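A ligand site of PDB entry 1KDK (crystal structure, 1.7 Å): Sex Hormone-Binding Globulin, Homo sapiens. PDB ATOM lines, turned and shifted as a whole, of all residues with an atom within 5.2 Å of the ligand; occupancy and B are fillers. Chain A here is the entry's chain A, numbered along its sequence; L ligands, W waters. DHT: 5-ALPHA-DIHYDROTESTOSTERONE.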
ATOM      1  N   THR A  29      -1.857  10.225 -33.594  1.00  0.00           N
ATOM      2  CA  THR A  29      -0.620   9.765 -32.950  1.00  0.00           C
ATOM      3  C   THR A  29      -0.598   8.240 -33.105  1.00  0.00           C
ATOM      4  O   THR A  29      -0.465   7.500 -32.127  1.00  0.00           O
ATOM      5  CB  THR A  29      -0.558  10.169 -31.455  1.00  0.00           C
ATOM      6  OG1 THR A  29      -1.774   9.653 -30.872  1.00  0.00           O
ATOM      7  CG2 THR A  29      -0.473  11.681 -31.246  1.00  0.00           C
ATOM      8  N   SER A  30      -0.575   7.798 -34.340  1.00  0.00           N
ATOM      9  CA  SER A  30      -0.501   6.392 -34.675  1.00  0.00           C
ATOM     10  C   SER A  30       0.137   6.191 -36.048  1.00  0.00           C
ATOM     11  O   SER A  30       0.345   7.111 -36.882  1.00  0.00           O
ATOM     12  CB  SER A  30      -1.899   5.765 -34.651  1.00  0.00           C
ATOM     13  OG  SER A  30      -2.600   6.167 -35.799  1.00  0.00           O
ATOM     14  N   SER A  31       0.664   4.983 -36.207  1.00  0.00           N
ATOM     15  CA  SER A  31       1.333   4.585 -37.431  1.00  0.00           C
ATOM     16  C   SER A  31       0.961   3.156 -37.802  1.00  0.00           C
ATOM     17  O   SER A  31       0.740   2.298 -36.953  1.00  0.00           O
ATOM     18  CB  SER A  31       2.846   4.778 -37.501  1.00  0.00           C
ATOM     19  OG  SER A  31       3.432   6.004 -37.144  1.00  0.00           O
ATOM     20  N   PHE A  45      11.258   0.180 -37.729  1.00  0.00           N
ATOM     21  CA  PHE A  45      11.330   1.648 -37.770  1.00  0.00           C
ATOM     22  C   PHE A  45      11.801   2.184 -36.446  1.00  0.00           C
ATOM     23  O   PHE A  45      11.810   1.549 -35.390  1.00  0.00           O
ATOM     24  CB  PHE A  45      10.036   2.376 -38.193  1.00  0.00           C
ATOM     25  CG  PHE A  45       8.995   2.563 -37.117  1.00  0.00           C
ATOM     26  CD1 PHE A  45       8.882   3.655 -36.271  1.00  0.00           C
ATOM     27  CD2 PHE A  45       8.051   1.565 -37.002  1.00  0.00           C
ATOM     28  CE1 PHE A  45       7.871   3.706 -35.324  1.00  0.00           C
ATOM     29  CE2 PHE A  45       7.005   1.567 -36.056  1.00  0.00           C
ATOM     30  CZ  PHE A  45       6.931   2.693 -35.236  1.00  0.00           C
ATOM     31  N   GLY A  47      12.042   6.001 -34.089  1.00  0.00           N
ATOM     32  CA  GLY A  47      11.477   7.394 -34.039  1.00  0.00           C
ATOM     33  C   GLY A  47      12.152   8.075 -32.874  1.00  0.00           C
ATOM     34  O   GLY A  47      12.453   7.470 -31.838  1.00  0.00           O
ATOM     35  N   ASP A  48      12.276   9.413 -32.981  1.00  0.00           N
ATOM     36  CA  ASP A  48      12.845  10.152 -31.853  1.00  0.00           C
ATOM     37  C   ASP A  48      12.474  11.651 -31.887  1.00  0.00           C
ATOM     38  O   ASP A  48      11.857  12.104 -32.827  1.00  0.00           O
ATOM     39  CB  ASP A  48      14.346   9.993 -31.769  1.00  0.00           C
ATOM     40  CG  ASP A  48      15.245  10.760 -32.758  1.00  0.00           C
ATOM     41  OD1 ASP A  48      14.779  11.793 -33.275  1.00  0.00           O
ATOM     42  OD2 ASP A  48      16.431  10.390 -32.899  1.00  0.00           O
ATOM     43  N   THR A  49      12.712  12.252 -30.738  1.00  0.00           N
ATOM     44  CA  THR A  49      12.775  13.714 -30.762  1.00  0.00           C
ATOM     45  C   THR A  49      14.224  14.054 -30.456  1.00  0.00           C
ATOM     46  O   THR A  49      14.808  15.101 -30.763  1.00  0.00           O
ATOM     47  CB  THR A  49      11.869  14.480 -29.811  1.00  0.00           C
ATOM     48  OG1 THR A  49      12.377  14.390 -28.465  1.00  0.00           O
ATOM     49  CG2 THR A  49      10.409  14.105 -29.933  1.00  0.00           C
ATOM     50  N   ASP A  54      15.280  10.650 -25.985  1.00  0.00           N
ATOM     51  CA  ASP A  54      13.832  10.480 -26.218  1.00  0.00           C
ATOM     52  C   ASP A  54      13.667   9.737 -27.533  1.00  0.00           C
ATOM     53  O   ASP A  54      13.514  10.340 -28.608  1.00  0.00           O
ATOM     54  CB  ASP A  54      13.227  11.877 -26.393  1.00  0.00           C
ATOM     55  CG  ASP A  54      11.725  11.876 -26.415  1.00  0.00           C
ATOM     56  OD1 ASP A  54      11.070  11.145 -25.627  1.00  0.00           O
ATOM     57  OD2 ASP A  54      11.140  12.555 -27.304  1.00  0.00           O
ATOM     58  N   TRP A  55      13.670   8.398 -27.500  1.00  0.00           N
ATOM     59  CA  TRP A  55      13.682   7.619 -28.731  1.00  0.00           C
ATOM     60  C   TRP A  55      12.948   6.279 -28.516  1.00  0.00           C
ATOM     61  O   TRP A  55      12.590   5.828 -27.416  1.00  0.00           O
ATOM     62  CB  TRP A  55      15.139   7.415 -29.202  1.00  0.00           C
ATOM     63  CG  TRP A  55      16.024   6.592 -28.320  1.00  0.00           C
ATOM     64  CD1 TRP A  55      16.903   7.133 -27.404  1.00  0.00           C
ATOM     65  CD2 TRP A  55      16.117   5.173 -28.207  1.00  0.00           C
ATOM     66  NE1 TRP A  55      17.616   6.111 -26.760  1.00  0.00           N
ATOM     67  CE2 TRP A  55      17.106   4.923 -27.240  1.00  0.00           C
ATOM     68  CE3 TRP A  55      15.513   4.098 -28.877  1.00  0.00           C
ATOM     69  CZ2 TRP A  55      17.404   3.588 -26.841  1.00  0.00           C
ATOM     70  CZ3 TRP A  55      15.815   2.773 -28.532  1.00  0.00           C
ATOM     71  CH2 TRP A  55      16.810   2.573 -27.556  1.00  0.00           C
ATOM     72  N   PHE A  56      12.616   5.687 -29.653  1.00  0.00           N
ATOM     73  CA  PHE A  56      11.833   4.494 -29.771  1.00  0.00           C
ATOM     74  C   PHE A  56      12.281   3.644 -30.956  1.00  0.00           C
ATOM     75  O   PHE A  56      12.498   4.167 -32.072  1.00  0.00           O
ATOM     76  CB  PHE A  56      10.362   4.849 -30.030  1.00  0.00           C
ATOM     77  CG  PHE A  56       9.370   3.756 -30.334  1.00  0.00           C
ATOM     78  CD1 PHE A  56       8.643   3.221 -29.239  1.00  0.00           C
ATOM     79  CD2 PHE A  56       9.171   3.242 -31.609  1.00  0.00           C
ATOM     80  CE1 PHE A  56       7.627   2.280 -29.513  1.00  0.00           C
ATOM     81  CE2 PHE A  56       8.209   2.252 -31.824  1.00  0.00           C
ATOM     82  CZ  PHE A  56       7.453   1.721 -30.779  1.00  0.00           C
ATOM     83  N   LEU A  69      12.602   1.517 -25.914  1.00  0.00           N
ATOM     84  CA  LEU A  69      12.119   2.916 -25.806  1.00  0.00           C
ATOM     85  C   LEU A  69      12.935   3.475 -24.678  1.00  0.00           C
ATOM     86  O   LEU A  69      13.283   2.810 -23.675  1.00  0.00           O
ATOM     87  CB  LEU A  69      10.640   2.714 -25.422  1.00  0.00           C
ATOM     88  CG  LEU A  69       9.624   3.712 -24.937  1.00  0.00           C
ATOM     89  CD1 LEU A  69       8.249   3.101 -25.181  1.00  0.00           C
ATOM     90  CD2 LEU A  69       9.880   4.074 -23.482  1.00  0.00           C
ATOM     91  N   ASN A  71      12.916   7.336 -22.687  1.00  0.00           N
ATOM     92  CA  ASN A  71      12.419   8.713 -22.631  1.00  0.00           C
ATOM     93  C   ASN A  71      12.471   9.090 -21.151  1.00  0.00           C
ATOM     94  O   ASN A  71      12.998   8.340 -20.343  1.00  0.00           O
ATOM     95  CB  ASN A  71      11.075   8.927 -23.338  1.00  0.00           C
ATOM     96  CG  ASN A  71       9.839   8.235 -22.841  1.00  0.00           C
ATOM     97  OD1 ASN A  71       8.848   8.063 -23.542  1.00  0.00           O
ATOM     98  ND2 ASN A  71       9.929   7.887 -21.578  1.00  0.00           N
ATOM     99  N   TRP A  73      10.077   9.190 -19.042  1.00  0.00           N
ATOM    100  CA  TRP A  73       9.217   8.363 -18.209  1.00  0.00           C
ATOM    101  C   TRP A  73       9.603   6.890 -18.110  1.00  0.00           C
ATOM    102  O   TRP A  73       9.193   6.203 -17.159  1.00  0.00           O
ATOM    103  CB  TRP A  73       7.780   8.387 -18.760  1.00  0.00           C
ATOM    104  CG  TRP A  73       7.279   9.804 -18.692  1.00  0.00           C
ATOM    105  CD1 TRP A  73       6.805  10.470 -17.599  1.00  0.00           C
ATOM    106  CD2 TRP A  73       7.412  10.766 -19.743  1.00  0.00           C
ATOM    107  NE1 TRP A  73       6.494  11.773 -17.946  1.00  0.00           N
ATOM    108  CE2 TRP A  73       6.848  11.969 -19.260  1.00  0.00           C
ATOM    109  CE3 TRP A  73       7.878  10.705 -21.052  1.00  0.00           C
ATOM    110  CZ2 TRP A  73       6.835  13.135 -20.031  1.00  0.00           C
ATOM    111  CZ3 TRP A  73       7.809  11.841 -21.841  1.00  0.00           C
ATOM    112  CH2 TRP A  73       7.286  13.036 -21.314  1.00  0.00           C
ATOM    113  N   VAL A  94       1.008   0.862 -34.526  1.00  0.00           N
ATOM    114  CA  VAL A  94       1.624   1.276 -33.261  1.00  0.00           C
ATOM    115  C   VAL A  94       0.925   2.589 -32.920  1.00  0.00           C
ATOM    116  O   VAL A  94       0.934   3.493 -33.773  1.00  0.00           O
ATOM    117  CB  VAL A  94       3.115   1.560 -33.418  1.00  0.00           C
ATOM    118  CG1 VAL A  94       3.715   2.052 -32.099  1.00  0.00           C
ATOM    119  CG2 VAL A  94       3.921   0.350 -33.843  1.00  0.00           C
ATOM    120  N   LYS A  95       0.330   2.642 -31.732  1.00  0.00           N
ATOM    121  CA  LYS A  95      -0.510   3.843 -31.484  1.00  0.00           C
ATOM    122  C   LYS A  95      -0.221   4.353 -30.090  1.00  0.00           C
ATOM    123  O   LYS A  95       0.049   3.534 -29.196  1.00  0.00           O
ATOM    124  CB  LYS A  95      -1.983   3.456 -31.522  1.00  0.00           C
ATOM    125  CG  LYS A  95      -2.664   2.501 -32.444  1.00  0.00           C
ATOM    126  CD  LYS A  95      -4.157   2.385 -32.131  1.00  0.00           C
ATOM    127  CE  LYS A  95      -4.760   1.395 -33.130  1.00  0.00           C
ATOM    128  NZ  LYS A  95      -6.174   1.767 -33.448  1.00  0.00           N
ATOM    129  N   MET A  96      -0.361   5.677 -29.928  1.00  0.00           N
ATOM    130  CA  MET A  96      -0.183   6.200 -28.566  1.00  0.00           C
ATOM    131  C   MET A  96      -1.602   6.536 -28.123  1.00  0.00           C
ATOM    132  O   MET A  96      -2.169   7.375 -28.848  1.00  0.00           O
ATOM    133  CB  MET A  96       0.669   7.451 -28.664  1.00  0.00           C
ATOM    134  CG  MET A  96       1.868   7.646 -27.794  1.00  0.00           C
ATOM    135  SD  MET A  96       2.181   9.327 -27.196  1.00  0.00           S
ATOM    136  CE  MET A  96       1.163  10.301 -28.311  1.00  0.00           C
ATOM    137  N   VAL A 101       1.562   3.186 -25.072  1.00  0.00           N
ATOM    138  CA  VAL A 101       1.898   2.869 -26.461  1.00  0.00           C
ATOM    139  C   VAL A 101       1.421   1.461 -26.692  1.00  0.00           C
ATOM    140  O   VAL A 101       1.763   0.571 -25.881  1.00  0.00           O
ATOM    141  CB  VAL A 101       3.427   3.013 -26.732  1.00  0.00           C
ATOM    142  CG1 VAL A 101       3.716   2.394 -28.124  1.00  0.00           C
ATOM    143  CG2 VAL A 101       3.866   4.461 -26.698  1.00  0.00           C
ATOM    144  N   SER A 117       4.432   7.685 -21.638  1.00  0.00           N
ATOM    145  CA  SER A 117       4.659   8.952 -22.385  1.00  0.00           C
ATOM    146  C   SER A 117       3.728  10.074 -21.988  1.00  0.00           C
ATOM    147  O   SER A 117       2.549   9.813 -21.843  1.00  0.00           O
ATOM    148  CB  SER A 117       4.354   8.665 -23.863  1.00  0.00           C
ATOM    149  OG  SER A 117       4.650   9.874 -24.592  1.00  0.00           O
ATOM    150  N   LEU A 120       2.162  14.463 -26.778  1.00  0.00           N
ATOM    151  CA  LEU A 120       3.048  14.932 -27.845  1.00  0.00           C
ATOM    152  C   LEU A 120       2.988  16.451 -27.905  1.00  0.00           C
ATOM    153  O   LEU A 120       4.035  17.105 -27.824  1.00  0.00           O
ATOM    154  CB  LEU A 120       2.771  14.258 -29.185  1.00  0.00           C
ATOM    155  CG  LEU A 120       3.187  12.792 -29.294  1.00  0.00           C
ATOM    156  CD1 LEU A 120       2.889  12.166 -30.651  1.00  0.00           C
ATOM    157  CD2 LEU A 120       4.661  12.620 -28.978  1.00  0.00           C
ATOM    158  N   LYS A 123       4.981  18.227 -25.239  1.00  0.00           N
ATOM    159  CA  LYS A 123       6.363  17.771 -25.124  1.00  0.00           C
ATOM    160  C   LYS A 123       7.410  18.758 -25.630  1.00  0.00           C
ATOM    161  O   LYS A 123       7.247  19.651 -26.462  1.00  0.00           O
ATOM    162  CB  LYS A 123       6.505  16.402 -25.779  1.00  0.00           C
ATOM    163  CG  LYS A 123       6.903  16.305 -27.235  1.00  0.00           C
ATOM    164  CD  LYS A 123       7.258  14.870 -27.617  1.00  0.00           C
ATOM    165  CE  LYS A 123       8.550  14.393 -26.973  1.00  0.00           C
ATOM    166  NZ  LYS A 123       8.312  13.131 -26.219  1.00  0.00           N
ATOM    167  N   MET A 128       9.542  15.590 -34.369  1.00  0.00           N
ATOM    168  CA  MET A 128       9.757  14.111 -34.235  1.00  0.00           C
ATOM    169  C   MET A 128      10.290  13.536 -35.537  1.00  0.00           C
ATOM    170  O   MET A 128       9.788  13.908 -36.611  1.00  0.00           O
ATOM    171  CB  MET A 128       8.395  13.471 -33.933  1.00  0.00           C
ATOM    172  CG  MET A 128       8.532  11.932 -33.778  1.00  0.00           C
ATOM    173  SD  MET A 128       7.029  11.324 -32.920  1.00  0.00           S
ATOM    174  CE  MET A 128       7.518  11.879 -31.280  1.00  0.00           C
ATOM    175  N   ILE A 130      10.947  10.078 -37.847  1.00  0.00           N
ATOM    176  CA  ILE A 130      10.622   8.682 -38.062  1.00  0.00           C
ATOM    177  C   ILE A 130      11.516   8.129 -39.183  1.00  0.00           C
ATOM    178  O   ILE A 130      11.553   8.668 -40.320  1.00  0.00           O
ATOM    179  CB  ILE A 130       9.152   8.476 -38.452  1.00  0.00           C
ATOM    180  CG1 ILE A 130       8.188   8.929 -37.346  1.00  0.00           C
ATOM    181  CG2 ILE A 130       8.889   7.005 -38.791  1.00  0.00           C
ATOM    182  CD1 ILE A 130       8.328   8.108 -36.070  1.00  0.00           C
ATOM    183  N   LEU A 160       2.300   8.648 -38.521  1.00  0.00           N
ATOM    184  CA  LEU A 160       1.782   9.782 -37.739  1.00  0.00           C
ATOM    185  C   LEU A 160       0.777  10.561 -38.595  1.00  0.00           C
ATOM    186  O   LEU A 160      -0.113  10.044 -39.245  1.00  0.00           O
ATOM    187  CB  LEU A 160       2.931  10.631 -37.210  1.00  0.00           C
ATOM    188  CG  LEU A 160       3.921  10.001 -36.236  1.00  0.00           C
ATOM    189  CD1 LEU A 160       5.173  10.835 -36.039  1.00  0.00           C
ATOM    190  CD2 LEU A 160       3.264   9.695 -34.889  1.00  0.00           C
HETATM  191  C1  DHT L   1       3.855   7.007 -31.121  1.00  0.00           C
HETATM  192  C2  DHT L   1       3.020   6.147 -32.092  1.00  0.00           C
HETATM  193  C3  DHT L   1       3.574   6.158 -33.483  1.00  0.00           C
HETATM  194  O3  DHT L   1       2.892   6.303 -34.510  1.00  0.00           O
HETATM  195  C4  DHT L   1       5.056   6.052 -33.629  1.00  0.00           C
HETATM  196  C5  DHT L   1       5.866   6.824 -32.620  1.00  0.00           C
HETATM  197  C6  DHT L   1       7.379   6.523 -32.677  1.00  0.00           C
HETATM  198  C7  DHT L   1       8.138   7.567 -31.848  1.00  0.00           C
HETATM  199  C8  DHT L   1       7.710   7.443 -30.358  1.00  0.00           C
HETATM  200  C9  DHT L   1       6.170   7.665 -30.272  1.00  0.00           C
HETATM  201  C10 DHT L   1       5.364   6.707 -31.155  1.00  0.00           C
HETATM  202  C11 DHT L   1       5.684   7.625 -28.783  1.00  0.00           C
HETATM  203  C12 DHT L   1       6.478   8.587 -27.894  1.00  0.00           C
HETATM  204  C13 DHT L   1       7.988   8.409 -28.039  1.00  0.00           C
HETATM  205  C14 DHT L   1       8.351   8.540 -29.527  1.00  0.00           C
HETATM  206  C15 DHT L   1       9.888   8.616 -29.518  1.00  0.00           C
HETATM  207  C16 DHT L   1      10.235   9.419 -28.237  1.00  0.00           C
HETATM  208  C17 DHT L   1       8.865   9.537 -27.546  1.00  0.00           C
HETATM  209  O17 DHT L   1       9.030   9.664 -26.107  1.00  0.00           O
HETATM  210  C18 DHT L   1       8.370   7.055 -27.421  1.00  0.00           C
HETATM  211  C19 DHT L   1       5.576   5.224 -30.713  1.00  0.00           C
HETATM  212  O   HOH W   1       6.873  11.146 -25.176  1.00  0.00           O
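Thr 29 touches the ligand.
C of Ser 30 touches O3 of the ligand (3.2 Å).
Phe 45 touches the ligand.
Gly 47 touches the ligand.
Trp 55 touches the ligand (N to C16, 3.7 Å).
Phe 56 touches the ligand.
Val 94 touches the ligand.
CG of Met 96 touches C1 of the ligand (3.9 Å).
OG of Ser 117 touches C12 of the ligand, at 3.99 Å.
Lys 123 touches the ligand.
Met 128 touches the ligand (CE to C14, 3.9 Å).
Ile 130 touches the ligand.
Leu 160 touches the ligand.
Hydrophobic or aromatic side chains within 4 Å of the ligand: Phe 45, Phe 56, Val 94, Met 96, Met 128, Ile 130 and Leu 160.
Of the 23 residues printed, 16 come within 4 Å of the ligand.
Water W1 lies within hydrogen-bond range of OG of Ser 117 (2.6 Å), NZ of Lys 123 (2.7 Å) and O17 of the ligand (2.8 Å).
The side-chain carboxylate of Asp 54 sits at hydrogen-bond distance from an oxygen (O17) of the ligand.
N of Ser 31 is in hydrogen-bond range of O3 of the ligand (3.1 Å).
An oxygen (O3) of the ligand is in hydrogen-bond range of the side-chain hydroxyl (OG) of Ser 31, at 2.7 Å.
An oxygen (O17) of the ligand sits at hydrogen-bond distance from the side-chain amide oxygen (OD1) of Asn 71, 3.0 Å away.
OD2 of Asp 54 is in salt-bridge range of NZ of Lys 123 (3.1 Å).
OD2 of Asp 54 is in hydrogen-bond range of OG1 of Thr 49 (2.5 Å).
OG of Ser 31 is in hydrogen-bond range of N of Leu 160 (3.2 Å).
The backbone carbonyl oxygen (O) of Ser 31 sits at hydrogen-bond distance from the backbone NH (N) of Val 94, at 2.8 Å.
ND2 of Asn 71 sits close to N of Trp 73 (2.9 Å).
N of Leu 160 lies within hydrogen-bond range of O of Ser 30 (3.0 Å).
The backbone NH (N) of Gly 47 sits at hydrogen-bond distance from the backbone carbonyl oxygen (O) of Phe 56 (2.8 Å).
OG of Ser 117 is in hydrogen-bond range of SD of Met 96 (3.6 Å).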
